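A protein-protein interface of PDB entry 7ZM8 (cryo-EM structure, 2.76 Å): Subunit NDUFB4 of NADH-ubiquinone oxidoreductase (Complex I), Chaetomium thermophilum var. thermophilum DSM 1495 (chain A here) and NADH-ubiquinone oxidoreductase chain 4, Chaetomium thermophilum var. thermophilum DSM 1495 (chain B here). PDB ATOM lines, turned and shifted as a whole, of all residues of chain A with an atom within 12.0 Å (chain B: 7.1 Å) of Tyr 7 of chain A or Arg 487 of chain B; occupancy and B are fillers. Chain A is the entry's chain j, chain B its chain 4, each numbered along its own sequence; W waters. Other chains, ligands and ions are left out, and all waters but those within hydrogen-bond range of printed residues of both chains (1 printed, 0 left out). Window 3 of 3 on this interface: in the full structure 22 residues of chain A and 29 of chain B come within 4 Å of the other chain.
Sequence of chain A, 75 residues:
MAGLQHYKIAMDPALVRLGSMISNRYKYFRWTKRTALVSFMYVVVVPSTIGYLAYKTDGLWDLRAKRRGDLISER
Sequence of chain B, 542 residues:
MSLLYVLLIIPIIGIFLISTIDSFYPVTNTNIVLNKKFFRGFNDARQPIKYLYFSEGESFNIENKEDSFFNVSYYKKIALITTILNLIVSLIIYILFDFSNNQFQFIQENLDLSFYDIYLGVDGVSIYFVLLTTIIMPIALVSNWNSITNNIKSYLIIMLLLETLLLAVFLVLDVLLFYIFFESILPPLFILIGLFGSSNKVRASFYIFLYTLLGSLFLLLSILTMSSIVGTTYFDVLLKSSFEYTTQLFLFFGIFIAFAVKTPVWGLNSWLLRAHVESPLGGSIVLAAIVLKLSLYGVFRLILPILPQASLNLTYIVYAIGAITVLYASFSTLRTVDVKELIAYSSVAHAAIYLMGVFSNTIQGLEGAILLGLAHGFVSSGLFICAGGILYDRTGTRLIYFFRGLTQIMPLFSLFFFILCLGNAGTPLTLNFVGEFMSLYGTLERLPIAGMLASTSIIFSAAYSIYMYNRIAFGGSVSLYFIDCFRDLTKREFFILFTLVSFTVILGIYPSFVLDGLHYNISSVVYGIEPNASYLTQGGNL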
ATOM      1  N   GLY A   3      18.811 -13.801  16.524  1.00  0.00           N
ATOM      2  CA  GLY A   3      17.451 -13.256  16.709  1.00  0.00           C
ATOM      3  C   GLY A   3      16.868 -12.679  15.437  1.00  0.00           C
ATOM      4  O   GLY A   3      16.895 -13.377  14.410  1.00  0.00           O
ATOM      5  N   LEU A   4      16.403 -11.430  15.464  1.00  0.00           N
ATOM      6  CA  LEU A   4      15.883 -10.772  14.234  1.00  0.00           C
ATOM      7  C   LEU A   4      17.014 -10.610  13.226  1.00  0.00           C
ATOM      8  O   LEU A   4      18.152 -10.374  13.648  1.00  0.00           O
ATOM      9  CB  LEU A   4      15.310  -9.381  14.528  1.00  0.00           C
ATOM     10  CG  LEU A   4      14.015  -9.306  15.325  1.00  0.00           C
ATOM     11  CD1 LEU A   4      12.981 -10.281  14.787  1.00  0.00           C
ATOM     12  CD2 LEU A   4      14.311  -9.583  16.778  1.00  0.00           C
ATOM     13  N   GLN A   5      16.699 -10.740  11.946  1.00  0.00           N
ATOM     14  CA  GLN A   5      17.728 -10.467  10.915  1.00  0.00           C
ATOM     15  C   GLN A   5      18.055  -8.982  10.966  1.00  0.00           C
ATOM     16  O   GLN A   5      17.135  -8.164  11.099  1.00  0.00           O
ATOM     17  CB  GLN A   5      17.262 -10.861   9.513  1.00  0.00           C
ATOM     18  CG  GLN A   5      15.888 -10.329   9.137  1.00  0.00           C
ATOM     19  CD  GLN A   5      15.643 -10.489   7.659  1.00  0.00           C
ATOM     20  OE1 GLN A   5      16.574 -10.487   6.855  1.00  0.00           O
ATOM     21  NE2 GLN A   5      14.381 -10.625   7.286  1.00  0.00           N
ATOM     22  N   HIS A   6      19.333  -8.669  10.859  1.00  0.00           N
ATOM     23  CA  HIS A   6      19.773  -7.265  10.884  1.00  0.00           C
ATOM     24  C   HIS A   6      20.054  -6.892   9.429  1.00  0.00           C
ATOM     25  O   HIS A   6      19.939  -7.776   8.577  1.00  0.00           O
ATOM     26  CB  HIS A   6      20.957  -7.160  11.845  1.00  0.00           C
ATOM     27  CG  HIS A   6      22.121  -8.020  11.491  1.00  0.00           C
ATOM     28  ND1 HIS A   6      23.239  -7.520  10.867  1.00  0.00           N
ATOM     29  CD2 HIS A   6      22.348  -9.335  11.675  1.00  0.00           C
ATOM     30  CE1 HIS A   6      24.104  -8.489  10.673  1.00  0.00           C
ATOM     31  NE2 HIS A   6      23.583  -9.612  11.158  1.00  0.00           N
ATOM     32  N   TYR A   7      20.365  -5.631   9.167  1.00  0.00           N
ATOM     33  CA  TYR A   7      20.716  -5.198   7.805  1.00  0.00           C
ATOM     34  C   TYR A   7      22.147  -5.662   7.532  1.00  0.00           C
ATOM     35  O   TYR A   7      22.829  -6.058   8.467  1.00  0.00           O
ATOM     36  CB  TYR A   7      20.589  -3.684   7.704  1.00  0.00           C
ATOM     37  CG  TYR A   7      19.199  -3.105   7.662  1.00  0.00           C
ATOM     38  CD1 TYR A   7      18.357  -3.359   6.598  1.00  0.00           C
ATOM     39  CD2 TYR A   7      18.750  -2.243   8.647  1.00  0.00           C
ATOM     40  CE1 TYR A   7      17.088  -2.816   6.536  1.00  0.00           C
ATOM     41  CE2 TYR A   7      17.488  -1.678   8.593  1.00  0.00           C
ATOM     42  CZ  TYR A   7      16.650  -1.971   7.535  1.00  0.00           C
ATOM     43  OH  TYR A   7      15.394  -1.445   7.456  1.00  0.00           O
ATOM     44  N   LYS A   8      22.586  -5.594   6.274  1.00  0.00           N
ATOM     45  CA  LYS A   8      23.944  -6.055   5.903  1.00  0.00           C
ATOM     46  C   LYS A   8      25.011  -5.036   6.292  1.00  0.00           C
ATOM     47  O   LYS A   8      24.879  -3.873   5.922  1.00  0.00           O
ATOM     48  CB  LYS A   8      23.986  -6.383   4.412  1.00  0.00           C
ATOM     49  CG  LYS A   8      23.086  -7.528   3.976  1.00  0.00           C
ATOM     50  CD  LYS A   8      23.136  -7.782   2.485  1.00  0.00           C
ATOM     51  CE  LYS A   8      22.150  -8.838   2.032  1.00  0.00           C
ATOM     52  NZ  LYS A   8      20.757  -8.458   2.360  1.00  0.00           N
ATOM     53  N   ILE A   9      26.034  -5.493   7.009  1.00  0.00           N
ATOM     54  CA  ILE A   9      27.163  -4.628   7.457  1.00  0.00           C
ATOM     55  C   ILE A   9      28.425  -5.249   6.875  1.00  0.00           C
ATOM     56  O   ILE A   9      28.540  -6.473   6.908  1.00  0.00           O
ATOM     57  CB  ILE A   9      27.235  -4.555   8.997  1.00  0.00           C
ATOM     58  CG1 ILE A   9      25.853  -4.422   9.636  1.00  0.00           C
ATOM     59  CG2 ILE A   9      28.164  -3.440   9.449  1.00  0.00           C
ATOM     60  CD1 ILE A   9      25.219  -3.084   9.394  1.00  0.00           C
ATOM     61  N   ALA A  10      29.309  -4.427   6.331  1.00  0.00           N
ATOM     62  CA  ALA A  10      30.587  -4.929   5.796  1.00  0.00           C
ATOM     63  C   ALA A  10      31.492  -5.092   7.000  1.00  0.00           C
ATOM     64  O   ALA A  10      32.226  -4.154   7.312  1.00  0.00           O
ATOM     65  CB  ALA A  10      31.150  -3.927   4.839  1.00  0.00           C
ATOM     66  N   MET A  11      31.395  -6.247   7.658  1.00  0.00           N
ATOM     67  CA  MET A  11      32.142  -6.445   8.916  1.00  0.00           C
ATOM     68  C   MET A  11      33.611  -6.533   8.576  1.00  0.00           C
ATOM     69  O   MET A  11      33.995  -7.418   7.804  1.00  0.00           O
ATOM     70  CB  MET A  11      31.696  -7.742   9.571  1.00  0.00           C
ATOM     71  CG  MET A  11      30.465  -7.552  10.427  1.00  0.00           C
ATOM     72  SD  MET A  11      30.852  -6.492  11.836  1.00  0.00           S
ATOM     73  CE  MET A  11      29.313  -5.602  12.023  1.00  0.00           C
ATOM     74  N   ASP A  12      34.389  -5.628   9.141  1.00  0.00           N
ATOM     75  CA  ASP A  12      35.815  -5.589   8.778  1.00  0.00           C
ATOM     76  C   ASP A  12      36.501  -6.705   9.562  1.00  0.00           C
ATOM     77  O   ASP A  12      36.471  -6.637  10.795  1.00  0.00           O
ATOM     78  CB  ASP A  12      36.399  -4.209   9.024  1.00  0.00           C
ATOM     79  CG  ASP A  12      37.809  -4.027   8.524  1.00  0.00           C
ATOM     80  OD1 ASP A  12      38.535  -5.021   8.406  1.00  0.00           O
ATOM     81  OD2 ASP A  12      38.147  -2.889   8.230  1.00  0.00           O
ATOM     82  N   ILE B 390      18.257  -0.194  19.115  1.00  0.00           N
ATOM     83  CA  ILE B 390      18.105   0.409  17.795  1.00  0.00           C
ATOM     84  C   ILE B 390      19.337   0.101  16.960  1.00  0.00           C
ATOM     85  O   ILE B 390      19.236  -0.498  15.887  1.00  0.00           O
ATOM     86  CB  ILE B 390      17.855   1.926  17.882  1.00  0.00           C
ATOM     87  CG1 ILE B 390      16.492   2.203  18.509  1.00  0.00           C
ATOM     88  CG2 ILE B 390      17.926   2.556  16.506  1.00  0.00           C
ATOM     89  CD1 ILE B 390      16.428   3.485  19.269  1.00  0.00           C
ATOM     90  N   ASP B 393      19.817  -3.787  17.000  1.00  0.00           N
ATOM     91  CA  ASP B 393      18.735  -4.356  16.166  1.00  0.00           C
ATOM     92  C   ASP B 393      19.072  -4.249  14.681  1.00  0.00           C
ATOM     93  O   ASP B 393      18.799  -5.213  13.969  1.00  0.00           O
ATOM     94  CB  ASP B 393      17.377  -3.726  16.479  1.00  0.00           C
ATOM     95  CG  ASP B 393      16.651  -4.414  17.621  1.00  0.00           C
ATOM     96  OD1 ASP B 393      17.318  -5.131  18.391  1.00  0.00           O
ATOM     97  OD2 ASP B 393      15.426  -4.228  17.725  1.00  0.00           O
ATOM     98  N   ARG B 394      19.654  -3.143  14.245  1.00  0.00           N
ATOM     99  CA  ARG B 394      19.901  -2.928  12.803  1.00  0.00           C
ATOM    100  C   ARG B 394      21.272  -3.411  12.348  1.00  0.00           C
ATOM    101  O   ARG B 394      21.424  -3.633  11.152  1.00  0.00           O
ATOM    102  CB  ARG B 394      19.807  -1.436  12.496  1.00  0.00           C
ATOM    103  CG  ARG B 394      18.385  -0.911  12.372  1.00  0.00           C
ATOM    104  CD  ARG B 394      18.321   0.559  12.740  1.00  0.00           C
ATOM    105  NE  ARG B 394      16.974   1.101  12.670  1.00  0.00           N
ATOM    106  CZ  ARG B 394      16.015   0.861  13.554  1.00  0.00           C
ATOM    107  NH1 ARG B 394      14.825   1.410  13.400  1.00  0.00           N
ATOM    108  NH2 ARG B 394      16.241   0.064  14.580  1.00  0.00           N
ATOM    109  N   THR B 395      22.226  -3.592  13.249  1.00  0.00           N
ATOM    110  CA  THR B 395      23.602  -3.891  12.780  1.00  0.00           C
ATOM    111  C   THR B 395      24.083  -5.218  13.321  1.00  0.00           C
ATOM    112  O   THR B 395      24.964  -5.793  12.690  1.00  0.00           O
ATOM    113  CB  THR B 395      24.571  -2.809  13.267  1.00  0.00           C
ATOM    114  OG1 THR B 395      24.597  -2.815  14.693  1.00  0.00           O
ATOM    115  CG2 THR B 395      24.200  -1.425  12.794  1.00  0.00           C
ATOM    116  N   GLY B 396      23.581  -5.631  14.479  1.00  0.00           N
ATOM    117  CA  GLY B 396      24.108  -6.845  15.114  1.00  0.00           C
ATOM    118  C   GLY B 396      25.465  -6.582  15.725  1.00  0.00           C
ATOM    119  O   GLY B 396      26.099  -7.542  16.156  1.00  0.00           O
ATOM    120  N   ILE B 409      20.630   9.690   7.874  1.00  0.00           N
ATOM    121  CA  ILE B 409      19.591   8.732   7.387  1.00  0.00           C
ATOM    122  C   ILE B 409      18.566   8.473   8.488  1.00  0.00           C
ATOM    123  O   ILE B 409      17.492   7.968   8.179  1.00  0.00           O
ATOM    124  CB  ILE B 409      20.262   7.423   6.918  1.00  0.00           C
ATOM    125  CG1 ILE B 409      21.247   6.878   7.955  1.00  0.00           C
ATOM    126  CG2 ILE B 409      20.912   7.606   5.557  1.00  0.00           C
ATOM    127  CD1 ILE B 409      21.587   5.426   7.772  1.00  0.00           C
ATOM    128  N   MET B 410      18.882   8.851   9.714  1.00  0.00           N
ATOM    129  CA  MET B 410      17.993   8.593  10.870  1.00  0.00           C
ATOM    130  C   MET B 410      17.886   9.866  11.701  1.00  0.00           C
ATOM    131  O   MET B 410      18.404   9.877  12.806  1.00  0.00           O
ATOM    132  CB  MET B 410      18.543   7.463  11.737  1.00  0.00           C
ATOM    133  CG  MET B 410      18.669   6.150  11.007  1.00  0.00           C
ATOM    134  SD  MET B 410      19.362   4.888  12.079  1.00  0.00           S
ATOM    135  CE  MET B 410      18.083   4.786  13.329  1.00  0.00           C
ATOM    136  N   PHE B 413      16.055   9.477  15.292  1.00  0.00           N
ATOM    137  CA  PHE B 413      16.901   8.847  16.294  1.00  0.00           C
ATOM    138  C   PHE B 413      17.920   9.833  16.847  1.00  0.00           C
ATOM    139  O   PHE B 413      18.158   9.875  18.056  1.00  0.00           O
ATOM    140  CB  PHE B 413      17.593   7.625  15.697  1.00  0.00           C
ATOM    141  CG  PHE B 413      18.740   7.120  16.515  1.00  0.00           C
ATOM    142  CD1 PHE B 413      18.514   6.412  17.678  1.00  0.00           C
ATOM    143  CD2 PHE B 413      20.045   7.356  16.125  1.00  0.00           C
ATOM    144  CE1 PHE B 413      19.562   5.946  18.435  1.00  0.00           C
ATOM    145  CE2 PHE B 413      21.096   6.896  16.882  1.00  0.00           C
ATOM    146  CZ  PHE B 413      20.853   6.188  18.039  1.00  0.00           C
ATOM    147  N   ILE B 483      26.276  -1.589   4.299  1.00  0.00           N
ATOM    148  CA  ILE B 483      26.104  -1.974   2.902  1.00  0.00           C
ATOM    149  C   ILE B 483      24.773  -1.465   2.368  1.00  0.00           C
ATOM    150  O   ILE B 483      24.684  -0.981   1.234  1.00  0.00           O
ATOM    151  CB  ILE B 483      26.230  -3.499   2.752  1.00  0.00           C
ATOM    152  CG1 ILE B 483      27.638  -3.947   3.122  1.00  0.00           C
ATOM    153  CG2 ILE B 483      25.899  -3.925   1.342  1.00  0.00           C
ATOM    154  CD1 ILE B 483      27.812  -5.430   3.116  1.00  0.00           C
ATOM    155  N   ASP B 484      23.726  -1.648   3.165  1.00  0.00           N
ATOM    156  CA  ASP B 484      22.374  -1.189   2.766  1.00  0.00           C
ATOM    157  C   ASP B 484      21.900  -0.088   3.719  1.00  0.00           C
ATOM    158  O   ASP B 484      22.492   0.041   4.789  1.00  0.00           O
ATOM    159  CB  ASP B 484      21.420  -2.382   2.697  1.00  0.00           C
ATOM    160  CG  ASP B 484      21.591  -3.371   3.831  1.00  0.00           C
ATOM    161  OD1 ASP B 484      22.039  -2.948   4.905  1.00  0.00           O
ATOM    162  OD2 ASP B 484      21.276  -4.554   3.622  1.00  0.00           O
ATOM    163  N   CYS B 485      20.907   0.700   3.315  1.00  0.00           N
ATOM    164  CA  CYS B 485      20.384   1.799   4.168  1.00  0.00           C
ATOM    165  C   CYS B 485      19.614   1.260   5.374  1.00  0.00           C
ATOM    166  O   CYS B 485      18.949   0.228   5.243  1.00  0.00           O
ATOM    167  CB  CYS B 485      19.508   2.773   3.396  1.00  0.00           C
ATOM    168  SG  CYS B 485      19.250   4.332   4.276  1.00  0.00           S
ATOM    169  N   PHE B 486      19.664   1.982   6.488  1.00  0.00           N
ATOM    170  CA  PHE B 486      18.931   1.571   7.703  1.00  0.00           C
ATOM    171  C   PHE B 486      17.665   2.398   7.792  1.00  0.00           C
ATOM    172  O   PHE B 486      17.739   3.597   7.536  1.00  0.00           O
ATOM    173  CB  PHE B 486      19.702   1.961   8.957  1.00  0.00           C
ATOM    174  CG  PHE B 486      20.951   1.164   9.201  1.00  0.00           C
ATOM    175  CD1 PHE B 486      21.300   0.120   8.362  1.00  0.00           C
ATOM    176  CD2 PHE B 486      21.769   1.458  10.274  1.00  0.00           C
ATOM    177  CE1 PHE B 486      22.451  -0.611   8.585  1.00  0.00           C
ATOM    178  CE2 PHE B 486      22.913   0.719  10.502  1.00  0.00           C
ATOM    179  CZ  PHE B 486      23.251  -0.309   9.657  1.00  0.00           C
ATOM    180  N   ARG B 487      16.553   1.782   8.186  1.00  0.00           N
ATOM    181  CA  ARG B 487      15.312   2.562   8.399  1.00  0.00           C
ATOM    182  C   ARG B 487      15.493   3.428   9.651  1.00  0.00           C
ATOM    183  O   ARG B 487      16.343   3.092  10.491  1.00  0.00           O
ATOM    184  CB  ARG B 487      14.110   1.624   8.539  1.00  0.00           C
ATOM    185  CG  ARG B 487      14.118   0.773   9.798  1.00  0.00           C
ATOM    186  CD  ARG B 487      12.961  -0.201   9.808  1.00  0.00           C
ATOM    187  NE  ARG B 487      11.680   0.432   9.535  1.00  0.00           N
ATOM    188  CZ  ARG B 487      10.526  -0.218   9.514  1.00  0.00           C
ATOM    189  NH1 ARG B 487       9.403   0.430   9.256  1.00  0.00           N
ATOM    190  NH2 ARG B 487      10.496  -1.515   9.754  1.00  0.00           N
ATOM    191  N   ASP B 488      14.698   4.489   9.776  1.00  0.00           N
ATOM    192  CA  ASP B 488      14.749   5.362  10.971  1.00  0.00           C
ATOM    193  C   ASP B 488      13.845   4.767  12.053  1.00  0.00           C
ATOM    194  O   ASP B 488      13.455   3.599  11.918  1.00  0.00           O
ATOM    195  CB  ASP B 488      14.420   6.809  10.593  1.00  0.00           C
ATOM    196  CG  ASP B 488      14.682   7.859  11.658  1.00  0.00           C
ATOM    197  OD1 ASP B 488      15.335   7.538  12.667  1.00  0.00           O
ATOM    198  OD2 ASP B 488      14.222   8.995  11.467  1.00  0.00           O
ATOM    199  N   LEU B 489      13.566   5.531  13.106  1.00  0.00           N
ATOM    200  CA  LEU B 489      12.772   5.054  14.258  1.00  0.00           C
ATOM    201  C   LEU B 489      11.411   4.506  13.839  1.00  0.00           C
ATOM    202  O   LEU B 489      10.787   5.092  12.945  1.00  0.00           O
ATOM    203  CB  LEU B 489      12.601   6.230  15.221  1.00  0.00           C
ATOM    204  CG  LEU B 489      13.799   6.529  16.117  1.00  0.00           C
ATOM    205  CD1 LEU B 489      13.375   7.381  17.301  1.00  0.00           C
ATOM    206  CD2 LEU B 489      14.444   5.240  16.597  1.00  0.00           C
ATOM    207  N   THR B 490      10.968   3.431  14.487  1.00  0.00           N
ATOM    208  CA  THR B 490       9.616   2.881  14.244  1.00  0.00           C
ATOM    209  C   THR B 490       8.678   3.647  15.156  1.00  0.00           C
ATOM    210  O   THR B 490       9.172   4.422  15.970  1.00  0.00           O
ATOM    211  CB  THR B 490       9.565   1.359  14.449  1.00  0.00           C
ATOM    212  OG1 THR B 490       9.864   1.035  15.805  1.00  0.00           O
ATOM    213  CG2 THR B 490      10.476   0.598  13.512  1.00  0.00           C
ATOM    214  N   LYS B 491       7.382   3.455  14.997  1.00  0.00           N
ATOM    215  CA  LYS B 491       6.383   4.157  15.821  1.00  0.00           C
ATOM    216  C   LYS B 491       6.514   3.515  17.198  1.00  0.00           C
ATOM    217  O   LYS B 491       6.219   4.185  18.177  1.00  0.00           O
ATOM    218  CB  LYS B 491       5.037   4.040  15.113  1.00  0.00           C
ATOM    219  CG  LYS B 491       3.851   4.786  15.690  1.00  0.00           C
ATOM    220  CD  LYS B 491       2.683   4.691  14.742  1.00  0.00           C
ATOM    221  CE  LYS B 491       1.427   5.350  15.260  1.00  0.00           C
ATOM    222  NZ  LYS B 491       0.926   4.665  16.468  1.00  0.00           N
ATOM    223  N   GLU B 493       9.651   2.487  18.476  1.00  0.00           N
ATOM    224  CA  GLU B 493      10.893   3.051  18.988  1.00  0.00           C
ATOM    225  C   GLU B 493      10.727   4.527  19.319  1.00  0.00           C
ATOM    226  O   GLU B 493      11.292   5.022  20.300  1.00  0.00           O
ATOM    227  CB  GLU B 493      12.012   2.861  17.967  1.00  0.00           C
ATOM    228  CG  GLU B 493      12.772   1.557  18.083  1.00  0.00           C
ATOM    229  CD  GLU B 493      13.404   1.134  16.766  1.00  0.00           C
ATOM    230  OE1 GLU B 493      12.836   1.446  15.706  1.00  0.00           O
ATOM    231  OE2 GLU B 493      14.454   0.466  16.789  1.00  0.00           O
HETATM  232  O   HOH W   1      17.924  -7.594  14.898  1.00  0.00           O
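Among the printed residues, merely in contact across the chains: Tyr 7 of chain A with Asp 484 of chain B, Ile 9 of chain A with Phe 486 of chain B, Ile 9 of chain A with Thr 395 of chain B, Tyr 7 of chain A with Arg 487 of chain B, Tyr 7 of chain A with Phe 486 of chain B, His 6 of chain A with Asp 393 of chain B, His 6 of chain A with Arg 394 of chain B, Ala 10 of chain A with Ile 483 of chain B, Tyr 7 of chain A with Cys 485 of chain B and Ile 9 of chain A with Ile 483 of chain B.
Water W1 lies within hydrogen-bond range of the backbone carbonyl oxygen (O) of Asp 393 of chain B (2.7 Å) and the backbone carbonyl oxygen (O) of Leu 4 of chain A (3.1 Å).
Hydrophobic or aromatic side chains of chain B that line the printed part of chain A: Ile 483 and Phe 486.
Among the printed residues, 14 pairs touch across the chains.
Tyr 7 of chain A touches five residues of chain B.
Arg 487 of chain B touches one residue of chain A.
Of chain A, only His 6 (3.6 Å) and Tyr 7 (3.0 Å) come within 4 Å of Arg 394 of chain B.
No residue of chain A comes within 4 Å of Met 410 of chain B.
Printed residues of chain A within 4 Å of Asp 484 of chain B: Tyr 7 (3.2 Å) and Lys 8 (3.0 Å).
Of chain A, only Tyr 7 (3.5 Å) and Ile 9 (3.4 Å) come within 4 Å of Phe 486 of chain B.
No residue of chain A comes within 4 Å of Asp 488 of chain B.
No residue of chain A comes within 4 Å of Thr 490 of chain B.
Of the printed residues of chain B, Ala 10 of chain A touches Ile 483.
Printed residues of chain B within 4 Å of Ile 9 of chain A: Thr 395, Ile 483 and Phe 486.
Met 11 of chain A touches none of the printed residues of chain B.
The nearest residue of chain B that does not touch Tyr 7 of chain A is Thr 395 of chain B (4.7 Å).
The nearest residue of chain A that does not touch Arg 487 of chain B is Gln 5 of chain A (9.1 Å).
A ring nitrogen (ND1) of His 6 of chain A is in hydrogen-bond range of the backbone carbonyl oxygen of Thr 395 of chain B.
N of Lys 8 of chain A is in hydrogen-bond range of OD1 of Asp 484 of chain B (3.0 Å).
N of Ile 483 of chain B is in hydrogen-bond range of O of Lys 8 of chain A.
O of Arg 394 of chain B lies within hydrogen-bond range of N of Tyr 7 of chain A.
NH2 of Arg 394 of chain B lies within salt-bridge range of OE2 of Glu 493 of chain B, at 2.9 Å.
The guanidinium group (NE) of Arg 394 of chain B sits at hydrogen-bond distance from the backbone carbonyl oxygen (O) of Arg 487 of chain B (3.0 Å).
The guanidinium group (NH1) of Arg 394 of chain B is in hydrogen-bond range of the backbone carbonyl oxygen (O) of Asp 488 of chain B.
The guanidinium group (NH2) of Arg 394 of chain B sits at hydrogen-bond distance from the backbone carbonyl oxygen (O) of Ile 390 of chain B (3.3 Å).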
